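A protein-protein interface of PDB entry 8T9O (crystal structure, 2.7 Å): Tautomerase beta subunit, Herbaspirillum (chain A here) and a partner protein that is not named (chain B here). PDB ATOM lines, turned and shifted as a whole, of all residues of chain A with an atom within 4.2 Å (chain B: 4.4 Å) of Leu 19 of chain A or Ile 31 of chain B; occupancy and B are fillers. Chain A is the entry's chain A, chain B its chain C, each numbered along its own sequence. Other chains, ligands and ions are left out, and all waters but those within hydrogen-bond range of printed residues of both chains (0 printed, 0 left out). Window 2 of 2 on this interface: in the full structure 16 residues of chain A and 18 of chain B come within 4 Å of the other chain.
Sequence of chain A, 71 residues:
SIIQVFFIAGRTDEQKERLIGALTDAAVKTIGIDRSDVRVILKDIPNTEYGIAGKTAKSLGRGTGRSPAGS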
ATOM      1  N   ARG A  11       2.555 -35.984 -14.596  1.00  0.00           N
ATOM      2  CA  ARG A  11       2.908 -34.612 -14.263  1.00  0.00           C
ATOM      3  C   ARG A  11       2.309 -33.646 -15.280  1.00  0.00           C
ATOM      4  O   ARG A  11       2.210 -33.950 -16.472  1.00  0.00           O
ATOM      5  CB  ARG A  11       4.426 -34.449 -14.206  1.00  0.00           C
ATOM      6  CG  ARG A  11       5.137 -35.592 -13.495  1.00  0.00           C
ATOM      7  CD  ARG A  11       5.566 -35.205 -12.086  1.00  0.00           C
ATOM      8  NE  ARG A  11       6.392 -36.238 -11.464  1.00  0.00           N
ATOM      9  CZ  ARG A  11       6.560 -36.375 -10.153  1.00  0.00           C
ATOM     10  NH1 ARG A  11       5.955 -35.546  -9.311  1.00  0.00           N
ATOM     11  NH2 ARG A  11       7.331 -37.345  -9.679  1.00  0.00           N
ATOM     12  N   GLN A  15       4.368 -28.450 -15.414  1.00  0.00           N
ATOM     13  CA  GLN A  15       5.488 -29.009 -14.660  1.00  0.00           C
ATOM     14  C   GLN A  15       6.584 -29.497 -15.595  1.00  0.00           C
ATOM     15  O   GLN A  15       7.775 -29.370 -15.289  1.00  0.00           O
ATOM     16  CB  GLN A  15       5.023 -30.154 -13.758  1.00  0.00           C
ATOM     17  CG  GLN A  15       4.522 -29.743 -12.384  1.00  0.00           C
ATOM     18  CD  GLN A  15       3.991 -30.925 -11.594  1.00  0.00           C
ATOM     19  OE1 GLN A  15       3.691 -31.978 -12.157  1.00  0.00           O
ATOM     20  NE2 GLN A  15       3.898 -30.763 -10.280  1.00  0.00           N
ATOM     21  N   LYS A  16       6.197 -30.065 -16.739  1.00  0.00           N
ATOM     22  CA  LYS A  16       7.184 -30.606 -17.665  1.00  0.00           C
ATOM     23  C   LYS A  16       8.040 -29.507 -18.275  1.00  0.00           C
ATOM     24  O   LYS A  16       9.249 -29.688 -18.457  1.00  0.00           O
ATOM     25  CB  LYS A  16       6.497 -31.414 -18.763  1.00  0.00           C
ATOM     26  CG  LYS A  16       6.123 -32.814 -18.339  1.00  0.00           C
ATOM     27  CD  LYS A  16       5.252 -33.480 -19.375  1.00  0.00           C
ATOM     28  CE  LYS A  16       4.803 -34.832 -18.889  1.00  0.00           C
ATOM     29  NZ  LYS A  16       3.347 -35.036 -19.100  1.00  0.00           N
ATOM     30  N   GLU A  17       7.441 -28.362 -18.603  1.00  0.00           N
ATOM     31  CA  GLU A  17       8.254 -27.281 -19.141  1.00  0.00           C
ATOM     32  C   GLU A  17       9.040 -26.577 -18.044  1.00  0.00           C
ATOM     33  O   GLU A  17      10.140 -26.077 -18.301  1.00  0.00           O
ATOM     34  CB  GLU A  17       7.398 -26.266 -19.898  1.00  0.00           C
ATOM     35  CG  GLU A  17       8.237 -25.404 -20.832  1.00  0.00           C
ATOM     36  CD  GLU A  17       7.468 -24.258 -21.455  1.00  0.00           C
ATOM     37  OE1 GLU A  17       6.373 -23.928 -20.954  1.00  0.00           O
ATOM     38  OE2 GLU A  17       7.965 -23.687 -22.449  1.00  0.00           O
ATOM     39  N   ARG A  18       8.500 -26.533 -16.822  1.00  0.00           N
ATOM     40  CA  ARG A  18       9.263 -25.988 -15.705  1.00  0.00           C
ATOM     41  C   ARG A  18      10.538 -26.795 -15.482  1.00  0.00           C
ATOM     42  O   ARG A  18      11.584 -26.236 -15.135  1.00  0.00           O
ATOM     43  CB  ARG A  18       8.401 -25.969 -14.441  1.00  0.00           C
ATOM     44  CG  ARG A  18       8.751 -24.860 -13.463  1.00  0.00           C
ATOM     45  CD  ARG A  18       7.947 -24.963 -12.173  1.00  0.00           C
ATOM     46  NE  ARG A  18       8.238 -23.854 -11.269  1.00  0.00           N
ATOM     47  CZ  ARG A  18       7.857 -23.799  -9.996  1.00  0.00           C
ATOM     48  NH1 ARG A  18       7.183 -24.805  -9.458  1.00  0.00           N
ATOM     49  NH2 ARG A  18       8.168 -22.743  -9.256  1.00  0.00           N
ATOM     50  N   LEU A  19      10.470 -28.111 -15.701  1.00  0.00           N
ATOM     51  CA  LEU A  19      11.638 -28.974 -15.541  1.00  0.00           C
ATOM     52  C   LEU A  19      12.663 -28.730 -16.640  1.00  0.00           C
ATOM     53  O   LEU A  19      13.858 -28.573 -16.362  1.00  0.00           O
ATOM     54  CB  LEU A  19      11.205 -30.439 -15.542  1.00  0.00           C
ATOM     55  CG  LEU A  19      12.181 -31.486 -14.999  1.00  0.00           C
ATOM     56  CD1 LEU A  19      12.467 -31.268 -13.517  1.00  0.00           C
ATOM     57  CD2 LEU A  19      11.642 -32.886 -15.253  1.00  0.00           C
ATOM     58  N   ILE A  20      12.212 -28.721 -17.899  1.00  0.00           N
ATOM     59  CA  ILE A  20      13.113 -28.534 -19.036  1.00  0.00           C
ATOM     60  C   ILE A  20      13.966 -27.288 -18.839  1.00  0.00           C
ATOM     61  O   ILE A  20      15.191 -27.316 -19.008  1.00  0.00           O
ATOM     62  CB  ILE A  20      12.309 -28.466 -20.348  1.00  0.00           C
ATOM     63  CG1 ILE A  20      11.854 -29.862 -20.781  1.00  0.00           C
ATOM     64  CG2 ILE A  20      13.124 -27.795 -21.444  1.00  0.00           C
ATOM     65  CD1 ILE A  20      10.818 -29.850 -21.886  1.00  0.00           C
ATOM     66  N   GLY A  21      13.330 -26.178 -18.463  1.00  0.00           N
ATOM     67  CA  GLY A  21      14.077 -24.953 -18.235  1.00  0.00           C
ATOM     68  C   GLY A  21      14.948 -25.015 -16.995  1.00  0.00           C
ATOM     69  O   GLY A  21      16.069 -24.498 -16.988  1.00  0.00           O
ATOM     70  N   ALA A  22      14.448 -25.647 -15.928  1.00  0.00           N
ATOM     71  CA  ALA A  22      15.207 -25.722 -14.683  1.00  0.00           C
ATOM     72  C   ALA A  22      16.481 -26.543 -14.842  1.00  0.00           C
ATOM     73  O   ALA A  22      17.517 -26.189 -14.264  1.00  0.00           O
ATOM     74  CB  ALA A  22      14.338 -26.311 -13.570  1.00  0.00           C
ATOM     75  N   LEU A  23      16.428 -27.630 -15.615  1.00  0.00           N
ATOM     76  CA  LEU A  23      17.600 -28.470 -15.812  1.00  0.00           C
ATOM     77  C   LEU A  23      18.612 -27.825 -16.750  1.00  0.00           C
ATOM     78  O   LEU A  23      19.822 -27.948 -16.527  1.00  0.00           O
ATOM     79  CB  LEU A  23      17.176 -29.831 -16.364  1.00  0.00           C
ATOM     80  CG  LEU A  23      16.401 -30.728 -15.395  1.00  0.00           C
ATOM     81  CD1 LEU A  23      15.731 -31.869 -16.144  1.00  0.00           C
ATOM     82  CD2 LEU A  23      17.304 -31.256 -14.289  1.00  0.00           C
ATOM     83  N   LEU A  42      12.422 -35.761 -21.944  1.00  0.00           N
ATOM     84  CA  LEU A  42      11.596 -36.264 -20.854  1.00  0.00           C
ATOM     85  C   LEU A  42      10.890 -37.538 -21.306  1.00  0.00           C
ATOM     86  O   LEU A  42      10.176 -37.535 -22.312  1.00  0.00           O
ATOM     87  CB  LEU A  42      10.588 -35.213 -20.391  1.00  0.00           C
ATOM     88  CG  LEU A  42      11.160 -33.843 -20.012  1.00  0.00           C
ATOM     89  CD1 LEU A  42      10.052 -32.909 -19.562  1.00  0.00           C
ATOM     90  CD2 LEU A  42      12.212 -33.974 -18.922  1.00  0.00           C
ATOM     91  N   THR B  27      15.190 -30.451 -10.137  1.00  0.00           N
ATOM     92  CA  THR B  27      14.020 -31.320 -10.128  1.00  0.00           C
ATOM     93  C   THR B  27      13.173 -31.110  -8.881  1.00  0.00           C
ATOM     94  O   THR B  27      11.952 -31.291  -8.924  1.00  0.00           O
ATOM     95  CB  THR B  27      14.451 -32.782 -10.220  1.00  0.00           C
ATOM     96  OG1 THR B  27      15.512 -32.904 -11.178  1.00  0.00           O
ATOM     97  CG2 THR B  27      13.290 -33.662 -10.643  1.00  0.00           C
ATOM     98  N   VAL B  28      13.805 -30.736  -7.768  1.00  0.00           N
ATOM     99  CA  VAL B  28      13.089 -30.555  -6.513  1.00  0.00           C
ATOM    100  C   VAL B  28      12.182 -29.348  -6.563  1.00  0.00           C
ATOM    101  O   VAL B  28      11.249 -29.221  -5.756  1.00  0.00           O
ATOM    102  CB  VAL B  28      14.109 -30.477  -5.360  1.00  0.00           C
ATOM    103  CG1 VAL B  28      13.516 -29.794  -4.118  1.00  0.00           C
ATOM    104  CG2 VAL B  28      14.608 -31.840  -5.022  1.00  0.00           C
ATOM    105  N   GLU B  29      12.402 -28.455  -7.499  1.00  0.00           N
ATOM    106  CA  GLU B  29      11.716 -27.183  -7.363  1.00  0.00           C
ATOM    107  C   GLU B  29      11.008 -26.716  -8.630  1.00  0.00           C
ATOM    108  O   GLU B  29      10.019 -25.990  -8.540  1.00  0.00           O
ATOM    109  CB  GLU B  29      12.786 -26.238  -6.776  1.00  0.00           C
ATOM    110  CG  GLU B  29      12.827 -24.813  -6.525  1.00  0.00           C
ATOM    111  CD  GLU B  29      11.633 -24.236  -5.931  1.00  0.00           C
ATOM    112  OE1 GLU B  29      10.534 -24.557  -6.415  1.00  0.00           O
ATOM    113  OE2 GLU B  29      11.859 -23.872  -4.678  1.00  0.00           O
ATOM    114  N   ALA B  30      11.383 -27.271  -9.788  1.00  0.00           N
ATOM    115  CA  ALA B  30      10.455 -27.330 -10.917  1.00  0.00           C
ATOM    116  C   ALA B  30       9.270 -28.256 -10.649  1.00  0.00           C
ATOM    117  O   ALA B  30       8.137 -27.910 -10.982  1.00  0.00           O
ATOM    118  CB  ALA B  30      11.194 -27.782 -12.176  1.00  0.00           C
ATOM    119  N   ILE B  31       9.517 -29.457 -10.120  1.00  0.00           N
ATOM    120  CA  ILE B  31       8.493 -30.426  -9.730  1.00  0.00           C
ATOM    121  C   ILE B  31       8.619 -30.557  -8.218  1.00  0.00           C
ATOM    122  O   ILE B  31       9.699 -30.332  -7.661  1.00  0.00           O
ATOM    123  CB  ILE B  31       8.678 -31.797 -10.436  1.00  0.00           C
ATOM    124  CG1 ILE B  31       8.510 -31.638 -11.955  1.00  0.00           C
ATOM    125  CG2 ILE B  31       7.725 -32.873  -9.919  1.00  0.00           C
ATOM    126  CD1 ILE B  31       8.867 -32.864 -12.772  1.00  0.00           C
ATOM    127  N   ASP B  32       7.517 -30.863  -7.526  1.00  0.00           N
ATOM    128  CA  ASP B  32       7.746 -30.939  -6.081  1.00  0.00           C
ATOM    129  C   ASP B  32       8.262 -32.312  -5.671  1.00  0.00           C
ATOM    130  O   ASP B  32       7.722 -32.952  -4.755  1.00  0.00           O
ATOM    131  CB  ASP B  32       6.514 -30.555  -5.264  1.00  0.00           C
ATOM    132  CG  ASP B  32       6.063 -29.129  -5.543  1.00  0.00           C
ATOM    133  OD1 ASP B  32       6.907 -28.336  -6.051  1.00  0.00           O
ATOM    134  OD2 ASP B  32       4.945 -28.782  -5.167  1.00  0.00           O
ATOM    135  N   ALA B  33       9.304 -32.787  -6.335  1.00  0.00           N
ATOM    136  CA  ALA B  33       9.834 -34.120  -6.087  1.00  0.00           C
ATOM    137  C   ALA B  33      10.790 -34.096  -4.899  1.00  0.00           C
ATOM    138  O   ALA B  33      11.617 -33.184  -4.794  1.00  0.00           O
ATOM    139  CB  ALA B  33      10.562 -34.645  -7.322  1.00  0.00           C
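Among the printed residues, merely in contact across the chains: Arg 11 of chain A with Ile 31 of chain B (3.3 Å), Arg 18 of chain A with Ala 30 of chain B (3.2 Å), Leu 19 of chain A with Thr 27 of chain B (3.7 Å), Leu 19 of chain A with Ala 30 of chain B (3.6 Å), Leu 19 of chain A with Ile 31 of chain B (3.7 Å), Ala 22 of chain A with Ala 30 of chain B (3.7 Å) and Leu 23 of chain A with Thr 27 of chain B (3.95 Å).
Of the 11 printed residues of chain A, 5 touch a printed residue of chain B.
Printed residues of chain A that touch a printed residue of chain B: Arg 11, Arg 18, Leu 19, Ala 22 and Leu 23.
Printed residues of chain B that touch a printed residue of chain A: Thr 27, Glu 29, Ala 30 and Ile 31.
Hydrophobic or aromatic side chains of chain B that line the printed part of chain A: Ala 30 and Ile 31.
Among the printed residues, 8 pairs touch across the chains.
Leu 19 of chain A touches just these residues of chain B: Thr 27 (3.7 Å), Ala 30 (3.6 Å) and Ile 31 (3.7 Å).
Ile 31 of chain B touches two residues of chain A.
Of the printed residues of chain A, Ala 30 of chain B touches Arg 18 (3.2 Å), Leu 19 (3.6 Å) and Ala 22 (3.7 Å).
Printed residues of chain A within 4 Å of Thr 27 of chain B: Leu 19 and Leu 23.
Printed residues of chain B within 4 Å of Arg 18 of chain A: Glu 29 (3.2 Å) and Ala 30 (3.2 Å).
Of the printed residues of chain B, Leu 23 of chain A touches Thr 27 (3.95 Å).
Printed residues of chain B within 4 Å of Arg 11 of chain A: Ile 31 (3.3 Å).
Val 28 of chain B touches none of the printed residues of chain A.
The nearest printed residue of chain B that does not touch Leu 19 of chain A is Val 28 of chain B (5.9 Å).
The nearest printed residue of chain A that does not touch Thr 27 of chain B is Ala 22 of chain A (5.4 Å).
NH1 of Arg 18 of chain A sits at hydrogen-bond distance from O of Glu 29 of chain B, at 3.2 Å.
NZ of Lys 16 of chain A is in hydrogen-bond range of O of Arg 11 of chain A.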
